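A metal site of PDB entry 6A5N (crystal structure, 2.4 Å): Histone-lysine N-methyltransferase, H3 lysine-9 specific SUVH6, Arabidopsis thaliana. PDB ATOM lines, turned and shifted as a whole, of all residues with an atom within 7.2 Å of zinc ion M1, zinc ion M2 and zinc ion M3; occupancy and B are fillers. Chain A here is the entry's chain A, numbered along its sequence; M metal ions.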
ATOM      1  N   LYS A 288      17.790  28.050 -19.677  1.00  0.00           N
ATOM      2  CA  LYS A 288      18.304  26.802 -19.125  1.00  0.00           C
ATOM      3  C   LYS A 288      17.420  25.645 -19.636  1.00  0.00           C
ATOM      4  O   LYS A 288      16.210  25.809 -19.771  1.00  0.00           O
ATOM      5  CB  LYS A 288      18.330  26.858 -17.592  1.00  0.00           C
ATOM      6  CG  LYS A 288      19.709  26.576 -16.955  1.00  0.00           C
ATOM      7  CD  LYS A 288      20.554  27.848 -16.846  1.00  0.00           C
ATOM      8  CE  LYS A 288      21.955  27.581 -16.293  1.00  0.00           C
ATOM      9  NZ  LYS A 288      22.644  26.492 -17.022  1.00  0.00           N
ATOM     10  N   SER A 289      18.044  24.500 -19.945  1.00  0.00           N
ATOM     11  CA  SER A 289      17.360  23.334 -20.531  1.00  0.00           C
ATOM     12  C   SER A 289      17.571  22.075 -19.686  1.00  0.00           C
ATOM     13  O   SER A 289      18.444  22.063 -18.817  1.00  0.00           O
ATOM     14  CB  SER A 289      17.879  23.090 -21.960  1.00  0.00           C
ATOM     15  OG  SER A 289      17.801  24.272 -22.739  1.00  0.00           O
ATOM     16  N   CYS A 290      16.778  21.022 -19.926  1.00  0.00           N
ATOM     17  CA  CYS A 290      16.948  19.752 -19.208  1.00  0.00           C
ATOM     18  C   CYS A 290      17.789  18.777 -20.011  1.00  0.00           C
ATOM     19  O   CYS A 290      17.966  18.946 -21.215  1.00  0.00           O
ATOM     20  CB  CYS A 290      15.582  19.126 -18.852  1.00  0.00           C
ATOM     21  SG  CYS A 290      14.638  18.391 -20.237  1.00  0.00           S
ATOM     22  N   CYS A 291      18.281  17.725 -19.350  1.00  0.00           N
ATOM     23  CA  CYS A 291      19.163  16.757 -19.981  1.00  0.00           C
ATOM     24  C   CYS A 291      18.528  15.369 -20.126  1.00  0.00           C
ATOM     25  O   CYS A 291      19.239  14.396 -20.381  1.00  0.00           O
ATOM     26  CB  CYS A 291      20.469  16.651 -19.180  1.00  0.00           C
ATOM     27  SG  CYS A 291      21.281  18.216 -18.891  1.00  0.00           S
ATOM     28  N   CYS A 292      17.214  15.282 -19.975  1.00  0.00           N
ATOM     29  CA  CYS A 292      16.538  13.993 -19.931  1.00  0.00           C
ATOM     30  C   CYS A 292      16.594  13.211 -21.261  1.00  0.00           C
ATOM     31  O   CYS A 292      16.357  13.777 -22.338  1.00  0.00           O
ATOM     32  CB  CYS A 292      15.090  14.179 -19.477  1.00  0.00           C
ATOM     33  SG  CYS A 292      14.864  14.871 -17.788  1.00  0.00           S
ATOM     34  N   THR A 293      16.924  11.925 -21.167  1.00  0.00           N
ATOM     35  CA  THR A 293      16.966  11.005 -22.313  1.00  0.00           C
ATOM     36  C   THR A 293      15.539  10.682 -22.752  1.00  0.00           C
ATOM     37  O   THR A 293      15.205  10.758 -23.938  1.00  0.00           O
ATOM     38  CB  THR A 293      17.672   9.666 -21.983  1.00  0.00           C
ATOM     39  OG1 THR A 293      16.877   8.914 -21.059  1.00  0.00           O
ATOM     40  CG2 THR A 293      19.060   9.897 -21.392  1.00  0.00           C
ATOM     41  N   THR A 294      14.729  10.301 -21.775  1.00  0.00           N
ATOM     42  CA  THR A 294      13.329   9.944 -21.973  1.00  0.00           C
ATOM     43  C   THR A 294      12.400  11.162 -21.791  1.00  0.00           C
ATOM     44  O   THR A 294      12.881  12.297 -21.730  1.00  0.00           O
ATOM     45  CB  THR A 294      12.911   8.823 -21.008  1.00  0.00           C
ATOM     46  OG1 THR A 294      11.530   8.466 -21.229  1.00  0.00           O
ATOM     47  CG2 THR A 294      13.094   9.274 -19.563  1.00  0.00           C
ATOM     48  N   ARG A 295      11.092  10.924 -21.722  1.00  0.00           N
ATOM     49  CA  ARG A 295      10.109  11.989 -21.496  1.00  0.00           C
ATOM     50  C   ARG A 295      10.192  12.543 -20.087  1.00  0.00           C
ATOM     51  O   ARG A 295      10.392  11.801 -19.122  1.00  0.00           O
ATOM     52  CB  ARG A 295       8.695  11.491 -21.771  1.00  0.00           C
ATOM     53  CG  ARG A 295       8.423  11.171 -23.223  1.00  0.00           C
ATOM     54  CD  ARG A 295       6.970  10.783 -23.420  1.00  0.00           C
ATOM     55  NE  ARG A 295       6.698   9.510 -22.765  1.00  0.00           N
ATOM     56  CZ  ARG A 295       5.895   8.574 -23.264  1.00  0.00           C
ATOM     57  NH1 ARG A 295       5.707   7.442 -22.599  1.00  0.00           N
ATOM     58  NH2 ARG A 295       5.291   8.772 -24.414  1.00  0.00           N
ATOM     59  N   CYS A 296      10.016  13.860 -19.952  1.00  0.00           N
ATOM     60  CA  CYS A 296      10.198  14.501 -18.659  1.00  0.00           C
ATOM     61  C   CYS A 296       8.984  14.304 -17.781  1.00  0.00           C
ATOM     62  O   CYS A 296       7.873  14.768 -18.089  1.00  0.00           O
ATOM     63  CB  CYS A 296      10.490  15.984 -18.841  1.00  0.00           C
ATOM     64  SG  CYS A 296      11.914  16.276 -19.884  1.00  0.00           S
ATOM     65  N   THR A 297       9.186  13.577 -16.689  1.00  0.00           N
ATOM     66  CA  THR A 297       8.107  13.324 -15.743  1.00  0.00           C
ATOM     67  C   THR A 297       8.660  13.437 -14.344  1.00  0.00           C
ATOM     68  O   THR A 297       9.875  13.330 -14.150  1.00  0.00           O
ATOM     69  CB  THR A 297       7.481  11.926 -15.929  1.00  0.00           C
ATOM     70  OG1 THR A 297       8.303  10.959 -15.266  1.00  0.00           O
ATOM     71  CG2 THR A 297       7.337  11.577 -17.391  1.00  0.00           C
ATOM     72  N   ARG A 302      15.884  10.287 -12.230  1.00  0.00           N
ATOM     73  CA  ARG A 302      16.613  11.511 -12.499  1.00  0.00           C
ATOM     74  C   ARG A 302      15.693  12.710 -12.517  1.00  0.00           C
ATOM     75  O   ARG A 302      14.615  12.675 -13.109  1.00  0.00           O
ATOM     76  CB  ARG A 302      17.379  11.427 -13.825  1.00  0.00           C
ATOM     77  CG  ARG A 302      18.494  10.377 -13.869  1.00  0.00           C
ATOM     78  CD  ARG A 302      19.057  10.283 -15.297  1.00  0.00           C
ATOM     79  NE  ARG A 302      18.827  11.548 -15.998  1.00  0.00           N
ATOM     80  CZ  ARG A 302      19.486  11.931 -17.088  1.00  0.00           C
ATOM     81  NH1 ARG A 302      20.405  11.147 -17.638  1.00  0.00           N
ATOM     82  NH2 ARG A 302      19.206  13.106 -17.636  1.00  0.00           N
ATOM     83  N   VAL A 303      16.126  13.774 -11.843  1.00  0.00           N
ATOM     84  CA  VAL A 303      15.392  15.027 -11.804  1.00  0.00           C
ATOM     85  C   VAL A 303      15.587  15.808 -13.099  1.00  0.00           C
ATOM     86  O   VAL A 303      16.655  15.737 -13.716  1.00  0.00           O
ATOM     87  CB  VAL A 303      15.834  15.867 -10.585  1.00  0.00           C
ATOM     88  CG1 VAL A 303      17.347  16.036 -10.556  1.00  0.00           C
ATOM     89  CG2 VAL A 303      15.149  17.212 -10.568  1.00  0.00           C
ATOM     90  N   CYS A 304      14.540  16.519 -13.509  1.00  0.00           N
ATOM     91  CA  CYS A 304      14.506  17.324 -14.732  1.00  0.00           C
ATOM     92  C   CYS A 304      14.467  18.806 -14.427  1.00  0.00           C
ATOM     93  O   CYS A 304      13.586  19.264 -13.701  1.00  0.00           O
ATOM     94  CB  CYS A 304      13.276  16.961 -15.572  1.00  0.00           C
ATOM     95  SG  CYS A 304      12.749  18.284 -16.715  1.00  0.00           S
ATOM     96  N   ALA A 305      15.394  19.570 -14.994  1.00  0.00           N
ATOM     97  CA  ALA A 305      15.480  21.006 -14.711  1.00  0.00           C
ATOM     98  C   ALA A 305      14.188  21.780 -15.014  1.00  0.00           C
ATOM     99  O   ALA A 305      13.881  22.775 -14.344  1.00  0.00           O
ATOM    100  CB  ALA A 305      16.632  21.600 -15.476  1.00  0.00           C
ATOM    101  N   CYS A 306      13.433  21.344 -16.036  1.00  0.00           N
ATOM    102  CA  CYS A 306      12.225  22.056 -16.421  1.00  0.00           C
ATOM    103  C   CYS A 306      11.058  21.722 -15.483  1.00  0.00           C
ATOM    104  O   CYS A 306      10.217  22.586 -15.185  1.00  0.00           O
ATOM    105  CB  CYS A 306      11.864  21.744 -17.872  1.00  0.00           C
ATOM    106  SG  CYS A 306      13.181  22.069 -19.101  1.00  0.00           S
ATOM    107  N   VAL A 307      11.021  20.492 -14.987  1.00  0.00           N
ATOM    108  CA  VAL A 307      10.133  20.126 -13.889  1.00  0.00           C
ATOM    109  C   VAL A 307      10.397  21.000 -12.659  1.00  0.00           C
ATOM    110  O   VAL A 307       9.498  21.680 -12.172  1.00  0.00           O
ATOM    111  CB  VAL A 307      10.312  18.634 -13.519  1.00  0.00           C
ATOM    112  CG1 VAL A 307       9.587  18.306 -12.222  1.00  0.00           C
ATOM    113  CG2 VAL A 307       9.778  17.776 -14.637  1.00  0.00           C
ATOM    114  N   LYS A 309      11.789  23.796 -12.574  1.00  0.00           N
ATOM    115  CA  LYS A 309      11.324  25.134 -12.938  1.00  0.00           C
ATOM    116  C   LYS A 309       9.803  25.296 -12.738  1.00  0.00           C
ATOM    117  O   LYS A 309       9.362  26.358 -12.306  1.00  0.00           O
ATOM    118  CB  LYS A 309      11.697  25.461 -14.386  1.00  0.00           C
ATOM    119  CG  LYS A 309      12.853  26.422 -14.510  1.00  0.00           C
ATOM    120  CD  LYS A 309      12.996  26.970 -15.918  1.00  0.00           C
ATOM    121  CE  LYS A 309      13.303  25.876 -16.920  1.00  0.00           C
ATOM    122  NZ  LYS A 309      13.674  26.393 -18.275  1.00  0.00           N
ATOM    123  N   GLU A 331       7.574  25.100 -20.592  1.00  0.00           N
ATOM    124  CA  GLU A 331       7.713  23.926 -21.442  1.00  0.00           C
ATOM    125  C   GLU A 331       9.193  23.650 -21.832  1.00  0.00           C
ATOM    126  O   GLU A 331      10.014  24.573 -21.824  1.00  0.00           O
ATOM    127  CB  GLU A 331       6.833  24.078 -22.685  1.00  0.00           C
ATOM    128  CG  GLU A 331       5.409  23.574 -22.457  1.00  0.00           C
ATOM    129  CD  GLU A 331       4.517  23.703 -23.679  1.00  0.00           C
ATOM    130  OE1 GLU A 331       4.922  23.210 -24.750  1.00  0.00           O
ATOM    131  OE2 GLU A 331       3.381  24.223 -23.542  1.00  0.00           O
ATOM    132  N   CYS A 332       9.504  22.387 -22.150  1.00  0.00           N
ATOM    133  CA  CYS A 332      10.854  22.009 -22.564  1.00  0.00           C
ATOM    134  C   CYS A 332      11.225  22.736 -23.858  1.00  0.00           C
ATOM    135  O   CYS A 332      10.435  22.776 -24.823  1.00  0.00           O
ATOM    136  CB  CYS A 332      10.951  20.494 -22.768  1.00  0.00           C
ATOM    137  SG  CYS A 332      11.219  19.514 -21.263  1.00  0.00           S
ATOM    138  N   GLY A 333      12.417  23.324 -23.882  1.00  0.00           N
ATOM    139  CA  GLY A 333      12.842  24.101 -25.037  1.00  0.00           C
ATOM    140  C   GLY A 333      13.509  23.298 -26.143  1.00  0.00           C
ATOM    141  O   GLY A 333      13.613  22.075 -26.059  1.00  0.00           O
ATOM    142  N   LEU A 335      16.574  23.308 -26.910  1.00  0.00           N
ATOM    143  CA  LEU A 335      17.882  22.809 -26.483  1.00  0.00           C
ATOM    144  C   LEU A 335      17.749  21.838 -25.290  1.00  0.00           C
ATOM    145  O   LEU A 335      18.746  21.438 -24.690  1.00  0.00           O
ATOM    146  CB  LEU A 335      18.808  23.988 -26.144  1.00  0.00           C
ATOM    147  CG  LEU A 335      19.202  24.850 -27.354  1.00  0.00           C
ATOM    148  CD1 LEU A 335      20.312  25.846 -27.035  1.00  0.00           C
ATOM    149  CD2 LEU A 335      19.600  23.970 -28.524  1.00  0.00           C
ATOM    150  N   CYS A 336      16.508  21.462 -24.973  1.00  0.00           N
ATOM    151  CA  CYS A 336      16.236  20.298 -24.132  1.00  0.00           C
ATOM    152  C   CYS A 336      16.458  19.042 -24.957  1.00  0.00           C
ATOM    153  O   CYS A 336      16.311  19.085 -26.176  1.00  0.00           O
ATOM    154  CB  CYS A 336      14.816  20.364 -23.586  1.00  0.00           C
ATOM    155  SG  CYS A 336      14.533  21.717 -22.433  1.00  0.00           S
ATOM    156  N   LYS A 337      16.813  17.924 -24.322  1.00  0.00           N
ATOM    157  CA  LYS A 337      17.240  16.717 -25.069  1.00  0.00           C
ATOM    158  C   LYS A 337      16.171  15.618 -25.154  1.00  0.00           C
ATOM    159  O   LYS A 337      16.410  14.543 -25.724  1.00  0.00           O
ATOM    160  CB  LYS A 337      18.514  16.166 -24.440  1.00  0.00           C
ATOM    161  CG  LYS A 337      19.776  16.967 -24.740  1.00  0.00           C
ATOM    162  CD  LYS A 337      20.060  17.005 -26.243  1.00  0.00           C
ATOM    163  CE  LYS A 337      20.910  18.220 -26.629  1.00  0.00           C
ATOM    164  NZ  LYS A 337      20.352  19.004 -27.778  1.00  0.00           N
ATOM    165  N   CYS A 338      15.013  15.905 -24.585  1.00  0.00           N
ATOM    166  CA  CYS A 338      13.845  15.032 -24.525  1.00  0.00           C
ATOM    167  C   CYS A 338      13.107  14.880 -25.852  1.00  0.00           C
ATOM    168  O   CYS A 338      13.058  15.842 -26.625  1.00  0.00           O
ATOM    169  CB  CYS A 338      12.874  15.599 -23.487  1.00  0.00           C
ATOM    170  SG  CYS A 338      12.581  17.362 -23.743  1.00  0.00           S
ATOM    171  N   PRO A 339      12.512  13.702 -26.112  1.00  0.00           N
ATOM    172  CA  PRO A 339      11.716  13.468 -27.318  1.00  0.00           C
ATOM    173  C   PRO A 339      10.522  14.428 -27.440  1.00  0.00           C
ATOM    174  O   PRO A 339      10.055  14.903 -26.407  1.00  0.00           O
ATOM    175  CB  PRO A 339      11.227  12.023 -27.147  1.00  0.00           C
ATOM    176  CG  PRO A 339      12.132  11.401 -26.160  1.00  0.00           C
ATOM    177  CD  PRO A 339      12.520  12.517 -25.221  1.00  0.00           C
ATOM    178  N   CYS A 342       7.532  14.251 -25.170  1.00  0.00           N
ATOM    179  CA  CYS A 342       7.625  14.698 -23.780  1.00  0.00           C
ATOM    180  C   CYS A 342       6.360  15.440 -23.336  1.00  0.00           C
ATOM    181  O   CYS A 342       5.817  16.278 -24.062  1.00  0.00           O
ATOM    182  CB  CYS A 342       8.855  15.589 -23.614  1.00  0.00           C
ATOM    183  SG  CYS A 342       8.893  16.514 -22.072  1.00  0.00           S
ATOM    184  N   TYR A 343       5.887  15.115 -22.139  1.00  0.00           N
ATOM    185  CA  TYR A 343       4.609  15.625 -21.663  1.00  0.00           C
ATOM    186  C   TYR A 343       4.723  17.127 -21.431  1.00  0.00           C
ATOM    187  O   TYR A 343       3.716  17.843 -21.400  1.00  0.00           O
ATOM    188  CB  TYR A 343       4.167  14.884 -20.393  1.00  0.00           C
ATOM    189  CG  TYR A 343       4.133  13.375 -20.530  1.00  0.00           C
ATOM    190  CD1 TYR A 343       3.250  12.750 -21.383  1.00  0.00           C
ATOM    191  CD2 TYR A 343       4.982  12.578 -19.784  1.00  0.00           C
ATOM    192  CE1 TYR A 343       3.219  11.370 -21.499  1.00  0.00           C
ATOM    193  CE2 TYR A 343       4.961  11.206 -19.895  1.00  0.00           C
ATOM    194  CZ  TYR A 343       4.080  10.608 -20.754  1.00  0.00           C
ATOM    195  OH  TYR A 343       4.059   9.233 -20.842  1.00  0.00           O
ATOM    196  N   LEU A 344       5.963  17.593 -21.269  1.00  0.00           N
ATOM    197  CA  LEU A 344       6.209  19.017 -21.066  1.00  0.00           C
ATOM    198  C   LEU A 344       6.368  19.729 -22.417  1.00  0.00           C
ATOM    199  O   LEU A 344       6.867  20.861 -22.487  1.00  0.00           O
ATOM    200  CB  LEU A 344       7.455  19.229 -20.177  1.00  0.00           C
ATOM    201  CG  LEU A 344       7.140  18.976 -18.703  1.00  0.00           C
ATOM    202  CD1 LEU A 344       8.288  19.324 -17.771  1.00  0.00           C
ATOM    203  CD2 LEU A 344       5.906  19.736 -18.293  1.00  0.00           C
ATOM    204  N   ARG A 345       5.912  19.066 -23.481  1.00  0.00           N
ATOM    205  CA  ARG A 345       5.692  19.705 -24.771  1.00  0.00           C
ATOM    206  C   ARG A 345       4.236  19.603 -25.179  1.00  0.00           C
ATOM    207  O   ARG A 345       3.780  18.509 -25.555  1.00  0.00           O
ATOM    208  CB  ARG A 345       6.565  19.066 -25.869  1.00  0.00           C
ATOM    209  CG  ARG A 345       8.010  18.837 -25.478  1.00  0.00           C
ATOM    210  CD  ARG A 345       8.888  18.771 -26.716  1.00  0.00           C
ATOM    211  NE  ARG A 345      10.276  18.481 -26.389  1.00  0.00           N
ATOM    212  CZ  ARG A 345      11.291  19.324 -26.585  1.00  0.00           C
ATOM    213  NH1 ARG A 345      12.523  18.965 -26.275  1.00  0.00           N
ATOM    214  NH2 ARG A 345      11.064  20.525 -27.089  1.00  0.00           N
HETATM  215 ZN    ZN M   1      13.687  16.957 -18.331  1.00  0.00          ZN
HETATM  216 ZN    ZN M   2      13.546  20.527 -20.590  1.00  0.00          ZN
HETATM  217 ZN    ZN M   3      11.342  17.436 -21.649  1.00  0.00          ZN
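Zinc ion M3 is bound by SG of Cys 332, SG of Cys 296, SG of Cys 338 and SG of Cys 342.
Four residues have an atom within 4 Å of zinc ion M2: Cys 290, Cys 306, Cys 332 and Cys 336.
Zinc ion M1 is bound by the side-chain sulfur (SG) of Cys 304 (2.3 Å), the side-chain sulfur (SG) of Cys 296 (2.5 Å), the side-chain sulfur (SG) of Cys 292 (2.5 Å) and the side-chain sulfur (SG) of Cys 290 (2.6 Å). Zinc ion M1 has four donor atoms within binding distance.
The nearest printed residue that does not touch zinc ion M3 is Leu 344 (4.5 Å).
NH2 of Arg 345 lies within hydrogen-bond range of O of Cys 332, at 3.3 Å. SG of Cys 304 lies close to N of Cys 306, at 3.2 Å. SG of Cys 304 sits close to N of Val 307 (3.3 Å). The backbone NH (N) of Gly 333 sits close to the side-chain sulfur (SG) of Cys 336, at 3.0 Å. The backbone NH (N) of Lys 337 sits at hydrogen-bond distance from the backbone carbonyl oxygen (O) of Cys 290 (3.5 Å). The backbone NH (N) of Cys 338 lies within hydrogen-bond range of the backbone carbonyl oxygen (O) of Cys 292, at 3.4 Å. The backbone carbonyl oxygen of Cys 338 lies within hydrogen-bond range of the guanidinium group of Arg 345, at 3.2 Å. The side-chain sulfur of Cys 342 lies close to the backbone NH of Leu 344, at 3.2 Å.
Four residues have an atom within 4 Å of zinc ion M1: Cys 290, Cys 292, Cys 296 and Cys 304. The nearest printed residue that does not touch zinc ion M1 is Ala 305 (4.6 Å).
Zinc ion M2 is bound by SG of Cys 306, 2.2 Å away. SG of Cys 336 is bound to zinc ion M2, at 2.4 Å. SG of Cys 290 binds zinc ion M2, at 2.4 Å. Zinc ion M2 is bound by SG of Cys 332 (2.6 Å). Zinc ion M2 has four donor atoms within binding distance.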
